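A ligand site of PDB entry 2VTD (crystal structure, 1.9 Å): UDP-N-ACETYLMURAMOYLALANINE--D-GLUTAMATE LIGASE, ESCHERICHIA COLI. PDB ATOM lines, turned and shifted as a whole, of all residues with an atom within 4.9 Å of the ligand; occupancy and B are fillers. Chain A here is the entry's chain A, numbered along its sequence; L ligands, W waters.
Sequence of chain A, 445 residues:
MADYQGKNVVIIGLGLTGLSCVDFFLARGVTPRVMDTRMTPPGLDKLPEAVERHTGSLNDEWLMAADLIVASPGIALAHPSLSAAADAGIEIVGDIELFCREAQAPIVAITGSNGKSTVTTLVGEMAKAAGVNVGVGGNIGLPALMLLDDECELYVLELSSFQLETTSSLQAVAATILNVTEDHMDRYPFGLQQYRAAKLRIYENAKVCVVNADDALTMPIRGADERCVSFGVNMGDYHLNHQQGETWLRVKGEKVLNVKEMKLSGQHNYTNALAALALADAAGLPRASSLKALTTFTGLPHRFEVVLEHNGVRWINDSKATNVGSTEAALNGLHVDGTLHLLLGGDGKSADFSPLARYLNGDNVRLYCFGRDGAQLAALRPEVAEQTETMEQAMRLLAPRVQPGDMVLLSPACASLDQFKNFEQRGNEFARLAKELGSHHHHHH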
ATOM      1  N   ILE A  12      35.777   3.392   5.662  1.00  0.00           N
ATOM      2  CA  ILE A  12      34.973   3.793   4.498  1.00  0.00           C
ATOM      3  C   ILE A  12      33.595   4.209   4.989  1.00  0.00           C
ATOM      4  O   ILE A  12      32.858   3.356   5.516  1.00  0.00           O
ATOM      5  CB  ILE A  12      34.820   2.643   3.504  1.00  0.00           C
ATOM      6  CG1 ILE A  12      36.172   2.048   3.124  1.00  0.00           C
ATOM      7  CG2 ILE A  12      34.056   3.088   2.236  1.00  0.00           C
ATOM      8  CD1 ILE A  12      36.049   1.026   2.001  1.00  0.00           C
ATOM      9  N   GLY A  13      33.259   5.483   4.864  1.00  0.00           N
ATOM     10  CA  GLY A  13      32.040   6.028   5.408  1.00  0.00           C
ATOM     11  C   GLY A  13      32.236   6.801   6.703  1.00  0.00           C
ATOM     12  O   GLY A  13      32.721   6.259   7.677  1.00  0.00           O
ATOM     13  N   MET A  35      37.694   7.556   3.998  1.00  0.00           N
ATOM     14  CA  MET A  35      37.173   7.923   2.673  1.00  0.00           C
ATOM     15  C   MET A  35      35.664   7.818   2.628  1.00  0.00           C
ATOM     16  O   MET A  35      35.073   7.095   3.451  1.00  0.00           O
ATOM     17  CB  MET A  35      37.777   7.085   1.535  1.00  0.00           C
ATOM     18  CG  MET A  35      37.504   5.582   1.608  1.00  0.00           C
ATOM     19  SD  MET A  35      38.363   4.688   0.307  1.00  0.00           S
ATOM     20  CE  MET A  35      39.991   5.348   0.577  1.00  0.00           C
ATOM     21  N   ASP A  36      35.031   8.539   1.697  1.00  0.00           N
ATOM     22  CA  ASP A  36      33.563   8.505   1.567  1.00  0.00           C
ATOM     23  C   ASP A  36      33.236   8.877   0.137  1.00  0.00           C
ATOM     24  O   ASP A  36      33.851   9.808  -0.419  1.00  0.00           O
ATOM     25  CB  ASP A  36      32.913   9.478   2.565  1.00  0.00           C
ATOM     26  CG  ASP A  36      31.422   9.219   2.780  1.00  0.00           C
ATOM     27  OD1 ASP A  36      30.633   9.234   1.813  1.00  0.00           O
ATOM     28  OD2 ASP A  36      31.043   8.987   3.923  1.00  0.00           O
ATOM     29  N   THR A  37      32.305   8.161  -0.466  1.00  0.00           N
ATOM     30  CA  THR A  37      31.901   8.442  -1.862  1.00  0.00           C
ATOM     31  C   THR A  37      31.165   9.792  -1.976  1.00  0.00           C
ATOM     32  O   THR A  37      31.079  10.360  -3.070  1.00  0.00           O
ATOM     33  CB  THR A  37      31.005   7.354  -2.443  1.00  0.00           C
ATOM     34  OG1 THR A  37      29.862   7.201  -1.614  1.00  0.00           O
ATOM     35  CG2 THR A  37      31.734   6.018  -2.517  1.00  0.00           C
ATOM     36  N   ARG A  38      30.670  10.293  -0.846  1.00  0.00           N
ATOM     37  CA  ARG A  38      29.970  11.574  -0.808  1.00  0.00           C
ATOM     38  C   ARG A  38      30.997  12.682  -0.678  1.00  0.00           C
ATOM     39  O   ARG A  38      31.958  12.568   0.103  1.00  0.00           O
ATOM     40  CB  ARG A  38      29.013  11.650   0.393  1.00  0.00           C
ATOM     41  CG  ARG A  38      27.888  10.605   0.408  1.00  0.00           C
ATOM     42  CD  ARG A  38      27.201  10.579   1.797  1.00  0.00           C
ATOM     43  NE  ARG A  38      28.038   9.929   2.827  1.00  0.00           N
ATOM     44  CZ  ARG A  38      27.604   9.499   4.018  1.00  0.00           C
ATOM     45  NH1 ARG A  38      26.333   9.637   4.390  1.00  0.00           N
ATOM     46  NH2 ARG A  38      28.451   8.934   4.856  1.00  0.00           N
ATOM     47  N   LEU A  58      35.815   6.592  -3.764  1.00  0.00           N
ATOM     48  CA  LEU A  58      36.772   5.741  -3.059  1.00  0.00           C
ATOM     49  C   LEU A  58      38.162   5.891  -3.673  1.00  0.00           C
ATOM     50  O   LEU A  58      38.298   5.963  -4.901  1.00  0.00           O
ATOM     51  CB  LEU A  58      36.348   4.277  -3.075  1.00  0.00           C
ATOM     52  CG  LEU A  58      34.972   3.977  -2.437  1.00  0.00           C
ATOM     53  CD1 LEU A  58      34.754   2.486  -2.310  1.00  0.00           C
ATOM     54  CD2 LEU A  58      34.833   4.661  -1.072  1.00  0.00           C
ATOM     55  N   SER A  72      31.680   1.068   6.615  1.00  0.00           N
ATOM     56  CA  SER A  72      30.392   1.514   7.125  1.00  0.00           C
ATOM     57  C   SER A  72      29.283   0.631   6.569  1.00  0.00           C
ATOM     58  O   SER A  72      29.380   0.167   5.428  1.00  0.00           O
ATOM     59  CB  SER A  72      30.113   2.943   6.676  1.00  0.00           C
ATOM     60  OG  SER A  72      28.723   3.211   6.895  1.00  0.00           O
ATOM     61  N   GLY A  74      26.725   1.459   5.372  1.00  0.00           N
ATOM     62  CA  GLY A  74      26.088   2.194   4.294  1.00  0.00           C
ATOM     63  C   GLY A  74      26.675   1.983   2.909  1.00  0.00           C
ATOM     64  O   GLY A  74      26.075   2.423   1.932  1.00  0.00           O
ATOM     65  N   ILE A  75      27.860   1.349   2.832  1.00  0.00           N
ATOM     66  CA  ILE A  75      28.486   0.969   1.555  1.00  0.00           C
ATOM     67  C   ILE A  75      28.433  -0.534   1.320  1.00  0.00           C
ATOM     68  O   ILE A  75      28.718  -1.338   2.219  1.00  0.00           O
ATOM     69  CB  ILE A  75      29.931   1.492   1.427  1.00  0.00           C
ATOM     70  CG1 ILE A  75      30.456   1.225  -0.003  1.00  0.00           C
ATOM     71  CG2 ILE A  75      30.901   0.882   2.468  1.00  0.00           C
ATOM     72  CD1 ILE A  75      31.441   2.217  -0.507  1.00  0.00           C
ATOM     73  N   ASN A 139      22.708  -0.333  15.826  1.00  0.00           N
ATOM     74  CA  ASN A 139      21.998   0.331  14.745  1.00  0.00           C
ATOM     75  C   ASN A 139      20.904   1.309  15.246  1.00  0.00           C
ATOM     76  O   ASN A 139      20.324   2.044  14.456  1.00  0.00           O
ATOM     77  CB  ASN A 139      21.418  -0.722  13.798  1.00  0.00           C
ATOM     78  CG  ASN A 139      20.975  -0.149  12.454  1.00  0.00           C
ATOM     79  OD1 ASN A 139      21.753   0.522  11.771  1.00  0.00           O
ATOM     80  ND2 ASN A 139      19.738  -0.454  12.055  1.00  0.00           N
ATOM     81  N   SER A 160      21.809  -4.408  12.085  1.00  0.00           N
ATOM     82  CA  SER A 160      21.215  -4.475  10.736  1.00  0.00           C
ATOM     83  C   SER A 160      21.821  -5.602   9.905  1.00  0.00           C
ATOM     84  O   SER A 160      22.924  -6.106  10.218  1.00  0.00           O
ATOM     85  CB  SER A 160      21.395  -3.161   9.997  1.00  0.00           C
ATOM     86  OG  SER A 160      22.764  -2.981   9.648  1.00  0.00           O
ATOM     87  N   PHE A 162      23.176  -5.256   7.140  1.00  0.00           N
ATOM     88  CA  PHE A 162      24.454  -4.723   6.615  1.00  0.00           C
ATOM     89  C   PHE A 162      25.606  -4.869   7.628  1.00  0.00           C
ATOM     90  O   PHE A 162      26.741  -5.211   7.258  1.00  0.00           O
ATOM     91  CB  PHE A 162      24.303  -3.252   6.222  1.00  0.00           C
ATOM     92  CG  PHE A 162      23.190  -2.976   5.198  1.00  0.00           C
ATOM     93  CD1 PHE A 162      22.852  -3.889   4.189  1.00  0.00           C
ATOM     94  CD2 PHE A 162      22.525  -1.747   5.221  1.00  0.00           C
ATOM     95  CE1 PHE A 162      21.822  -3.574   3.253  1.00  0.00           C
ATOM     96  CE2 PHE A 162      21.520  -1.419   4.283  1.00  0.00           C
ATOM     97  CZ  PHE A 162      21.164  -2.366   3.310  1.00  0.00           C
ATOM     98  N   ASP A 183      13.002  -5.988   2.159  1.00  0.00           N
ATOM     99  CA  ASP A 183      13.622  -4.720   2.504  1.00  0.00           C
ATOM    100  C   ASP A 183      15.022  -4.730   1.911  1.00  0.00           C
ATOM    101  O   ASP A 183      15.588  -5.806   1.649  1.00  0.00           O
ATOM    102  CB  ASP A 183      13.688  -4.532   4.033  1.00  0.00           C
ATOM    103  CG  ASP A 183      13.911  -3.086   4.454  1.00  0.00           C
ATOM    104  OD1 ASP A 183      13.997  -2.185   3.585  1.00  0.00           O
ATOM    105  OD2 ASP A 183      13.958  -2.846   5.702  1.00  0.00           O
ATOM    106  N   HIS A 184      15.576  -3.543   1.683  1.00  0.00           N
ATOM    107  CA  HIS A 184      16.988  -3.374   1.275  1.00  0.00           C
ATOM    108  C   HIS A 184      17.312  -4.075  -0.048  1.00  0.00           C
ATOM    109  O   HIS A 184      18.454  -4.510  -0.265  1.00  0.00           O
ATOM    110  CB  HIS A 184      17.907  -3.929   2.379  1.00  0.00           C
ATOM    111  CG  HIS A 184      17.678  -3.305   3.716  1.00  0.00           C
ATOM    112  ND1 HIS A 184      17.839  -1.964   3.936  1.00  0.00           N
ATOM    113  CD2 HIS A 184      17.280  -3.841   4.896  1.00  0.00           C
ATOM    114  CE1 HIS A 184      17.562  -1.697   5.202  1.00  0.00           C
ATOM    115  NE2 HIS A 184      17.242  -2.825   5.811  1.00  0.00           N
ATOM    116  N   THR A 322       9.945   2.027   7.561  1.00  0.00           N
ATOM    117  CA  THR A 322      10.799   2.297   6.412  1.00  0.00           C
ATOM    118  C   THR A 322      10.748   1.164   5.386  1.00  0.00           C
ATOM    119  O   THR A 322      11.554   1.148   4.461  1.00  0.00           O
ATOM    120  CB  THR A 322      12.259   2.509   6.895  1.00  0.00           C
ATOM    121  OG1 THR A 322      12.610   1.429   7.774  1.00  0.00           O
ATOM    122  CG2 THR A 322      12.390   3.812   7.685  1.00  0.00           C
ATOM    123  N   LYS A 349      13.605   1.658  -2.026  1.00  0.00           N
ATOM    124  CA  LYS A 349      14.611   0.575  -2.048  1.00  0.00           C
ATOM    125  C   LYS A 349      14.200  -0.623  -2.936  1.00  0.00           C
ATOM    126  O   LYS A 349      14.431  -1.797  -2.587  1.00  0.00           O
ATOM    127  CB  LYS A 349      14.954   0.120  -0.607  1.00  0.00           C
ATOM    128  CG  LYS A 349      15.561   1.227   0.253  1.00  0.00           C
ATOM    129  CD  LYS A 349      15.615   0.871   1.728  1.00  0.00           C
ATOM    130  CE  LYS A 349      14.247   1.182   2.421  1.00  0.00           C
ATOM    131  NZ  LYS A 349      14.154   0.548   3.769  1.00  0.00           N
ATOM    132  N   ALA A 415      12.448   4.359   3.010  1.00  0.00           N
ATOM    133  CA  ALA A 415      13.485   5.185   3.588  1.00  0.00           C
ATOM    134  C   ALA A 415      13.287   6.689   3.348  1.00  0.00           C
ATOM    135  O   ALA A 415      12.636   7.083   2.413  1.00  0.00           O
ATOM    136  CB  ALA A 415      14.837   4.741   3.073  1.00  0.00           C
ATOM    137  N   SER A 416      13.901   7.507   4.188  1.00  0.00           N
ATOM    138  CA  SER A 416      13.692   8.981   4.093  1.00  0.00           C
ATOM    139  C   SER A 416      14.848   9.641   3.381  1.00  0.00           C
ATOM    140  O   SER A 416      14.857  10.852   3.132  1.00  0.00           O
ATOM    141  CB  SER A 416      13.610   9.566   5.476  1.00  0.00           C
ATOM    142  OG  SER A 416      14.806   9.371   6.179  1.00  0.00           O
ATOM    143  N   LEU A 417      15.831   8.824   3.039  1.00  0.00           N
ATOM    144  CA  LEU A 417      17.187   9.317   2.708  1.00  0.00           C
ATOM    145  C   LEU A 417      17.263  10.101   1.391  1.00  0.00           C
ATOM    146  O   LEU A 417      18.278  10.740   1.101  1.00  0.00           O
ATOM    147  CB  LEU A 417      18.178   8.136   2.711  1.00  0.00           C
ATOM    148  CG  LEU A 417      18.316   7.443   4.076  1.00  0.00           C
ATOM    149  CD1 LEU A 417      19.378   6.340   4.010  1.00  0.00           C
ATOM    150  CD2 LEU A 417      18.629   8.418   5.221  1.00  0.00           C
ATOM    151  N   ASN A 422      17.566  11.323   8.030  1.00  0.00           N
ATOM    152  CA  ASN A 422      17.185  10.013   8.531  1.00  0.00           C
ATOM    153  C   ASN A 422      15.687  10.030   8.870  1.00  0.00           C
ATOM    154  O   ASN A 422      15.037  11.095   8.836  1.00  0.00           O
ATOM    155  CB  ASN A 422      18.012   9.640   9.773  1.00  0.00           C
ATOM    156  CG  ASN A 422      18.065  10.767  10.776  1.00  0.00           C
ATOM    157  OD1 ASN A 422      17.023  11.299  11.215  1.00  0.00           O
ATOM    158  ND2 ASN A 422      19.271  11.187  11.101  1.00  0.00           N
ATOM    159  N   PHE A 423      15.125   8.867   9.184  1.00  0.00           N
ATOM    160  CA  PHE A 423      13.725   8.797   9.523  1.00  0.00           C
ATOM    161  C   PHE A 423      13.368   9.673  10.749  1.00  0.00           C
ATOM    162  O   PHE A 423      12.213  10.022  10.931  1.00  0.00           O
ATOM    163  CB  PHE A 423      13.292   7.350   9.721  1.00  0.00           C
ATOM    164  CG  PHE A 423      13.753   6.769  11.026  1.00  0.00           C
ATOM    165  CD1 PHE A 423      13.033   6.987  12.211  1.00  0.00           C
ATOM    166  CD2 PHE A 423      14.926   5.991  11.080  1.00  0.00           C
ATOM    167  CE1 PHE A 423      13.479   6.489  13.416  1.00  0.00           C
ATOM    168  CE2 PHE A 423      15.383   5.475  12.298  1.00  0.00           C
ATOM    169  CZ  PHE A 423      14.647   5.704  13.458  1.00  0.00           C
ATOM    170  N   ARG A 426      12.617  13.097   9.512  1.00  0.00           N
ATOM    171  CA  ARG A 426      11.295  13.018   8.862  1.00  0.00           C
ATOM    172  C   ARG A 426      10.128  13.024   9.880  1.00  0.00           C
ATOM    173  O   ARG A 426       9.150  13.753   9.672  1.00  0.00           O
ATOM    174  CB  ARG A 426      11.217  11.766   7.967  1.00  0.00           C
ATOM    175  CG  ARG A 426       9.871  11.584   7.289  1.00  0.00           C
ATOM    176  CD  ARG A 426       9.907  10.433   6.309  1.00  0.00           C
ATOM    177  NE  ARG A 426      10.159   9.120   6.944  1.00  0.00           N
ATOM    178  CZ  ARG A 426      10.422   7.999   6.249  1.00  0.00           C
ATOM    179  NH1 ARG A 426      10.538   8.005   4.919  1.00  0.00           N
ATOM    180  NH2 ARG A 426      10.594   6.857   6.907  1.00  0.00           N
HETATM  181  N1  LIG L   1      31.433   5.484   1.575  1.00  0.00           N
HETATM  182  C1  LIG L   1      30.335   5.688   1.837  1.00  0.00           C
HETATM  183  C2  LIG L   1      29.105   5.960   2.046  1.00  0.00           C
HETATM  184  C3  LIG L   1      28.439   5.682   3.239  1.00  0.00           C
HETATM  185  C4  LIG L   1      27.088   6.024   3.363  1.00  0.00           C
HETATM  186  C5  LIG L   1      28.415   6.582   1.022  1.00  0.00           C
HETATM  187  C6  LIG L   1      27.079   6.916   1.161  1.00  0.00           C
HETATM  188  C7  LIG L   1      26.433   6.640   2.317  1.00  0.00           C
HETATM  189  C8  LIG L   1      24.981   7.022   2.371  1.00  0.00           C
HETATM  190  O1  LIG L   1      24.461   6.531   3.576  1.00  0.00           O
HETATM  191  C9  LIG L   1      23.540   5.535   3.736  1.00  0.00           C
HETATM  192  C10 LIG L   1      22.747   4.939   2.756  1.00  0.00           C
HETATM  193  C11 LIG L   1      21.853   3.926   3.131  1.00  0.00           C
HETATM  194  C12 LIG L   1      23.422   5.139   5.027  1.00  0.00           C
HETATM  195  C13 LIG L   1      22.554   4.164   5.387  1.00  0.00           C
HETATM  196  C14 LIG L   1      21.760   3.534   4.461  1.00  0.00           C
HETATM  197  C15 LIG L   1      20.896   2.550   4.902  1.00  0.00           C
HETATM  198  C16 LIG L   1      22.534   3.844   6.720  1.00  0.00           C
HETATM  199  C17 LIG L   1      21.669   2.875   7.145  1.00  0.00           C
HETATM  200  C18 LIG L   1      20.868   2.232   6.238  1.00  0.00           C
HETATM  201  S1  LIG L   1      19.890   1.170   6.848  1.00  0.00           S
HETATM  202  O2  LIG L   1      19.443   0.271   5.796  1.00  0.00           O
HETATM  203  O3  LIG L   1      20.464   0.465   7.974  1.00  0.00           O
HETATM  204  N2  LIG L   1      18.751   1.968   7.443  1.00  0.00           N
HETATM  205  C19 LIG L   1      17.830   2.721   6.598  1.00  0.00           C
HETATM  206  C20 LIG L   1      16.708   1.866   6.077  1.00  0.00           C
HETATM  207  O4  LIG L   1      16.223   1.020   6.821  1.00  0.00           O
HETATM  208  O5  LIG L   1      16.323   2.062   4.920  1.00  0.00           O
HETATM  209  C21 LIG L   1      17.289   3.892   7.426  1.00  0.00           C
HETATM  210  C22 LIG L   1      16.467   4.825   6.549  1.00  0.00           C
HETATM  211  C23 LIG L   1      16.035   6.122   7.194  1.00  0.00           C
HETATM  212  O6  LIG L   1      16.587   6.542   8.203  1.00  0.00           O
HETATM  213  O7  LIG L   1      15.110   6.722   6.637  1.00  0.00           O
HETATM  214  F1  LIG L   1      26.398   7.514   0.180  1.00  0.00           F
HETATM  215  O   HOH W   1      14.049  -0.471   6.579  1.00  0.00           O
HETATM  216  O   HOH W   2      23.129  -0.283   9.234  1.00  0.00           O
HETATM  217  O   HOH W   3      18.395   5.952   9.948  1.00  0.00           O
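Water W1 lies within hydrogen-bond range of OD2 of Asp 183 (2.5 Å), O4 of the ligand (2.6 Å), OG1 of Thr 322 (2.7 Å) and NZ of Lys 349 (3.0 Å).
Water W2 lies within hydrogen-bond range of the side-chain hydroxyl (OG) of Ser 160, the side-chain amide oxygen (OD1) of Asn 139 and an oxygen (O3) of the ligand.
NH2 of Arg 38 is in salt-bridge range of OD2 of Asp 36 (2.8 Å).
The side-chain amino group (NZ) of Lys 349 is in hydrogen-bond range of the backbone carbonyl oxygen (O) of Thr 322.
The backbone carbonyl oxygen (O) of Asn 422 lies close to the side-chain hydroxyl (OG) of Ser 416 (3.2 Å).
OD2 of Asp 183 is in hydrogen-bond range of NE2 of His 184 (3.3 Å).
N of Gly 13 lies within hydrogen-bond range of O of Met 35 (2.8 Å).
The side-chain amino group (NZ) of Lys 349 is in salt-bridge range of the side-chain carboxylate (OD1) of Asp 183 (2.7 Å).
OG of Ser 160 sits close to N of Phe 162, at 3.4 Å.
NH1 of Arg 426 sits at hydrogen-bond distance from O of Ala 415 (3.4 Å).
Residues that only touch the ligand: Phe 162, Arg 38, Asn 422, Asp 36, Leu 417, Ala 415, Ile 12, Thr 322, Gly 13 and Ile 75.
Of the 23 residues printed, 15 come within 4 Å of the ligand.
The nearest printed residue that does not touch the ligand is Gly 74 (4.01 Å).
An oxygen (O5) of the ligand lies within salt-bridge range of the side-chain amino group (NZ) of Lys 349 (2.9 Å).
N of Thr 37 lies within hydrogen-bond range of N1 of the ligand, at 3.5 Å.
An oxygen (O2) of the ligand sits close to a ring nitrogen (ND1) of His 184.
The side-chain hydroxyl (OG) of Ser 416 lies within hydrogen-bond range of an oxygen (O7) of the ligand (2.7 Å).
The backbone NH (N) of Ser 416 is in hydrogen-bond range of an oxygen (O7) of the ligand (2.8 Å).
The backbone NH of Phe 423 is in hydrogen-bond range of an oxygen (O6) of the ligand.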
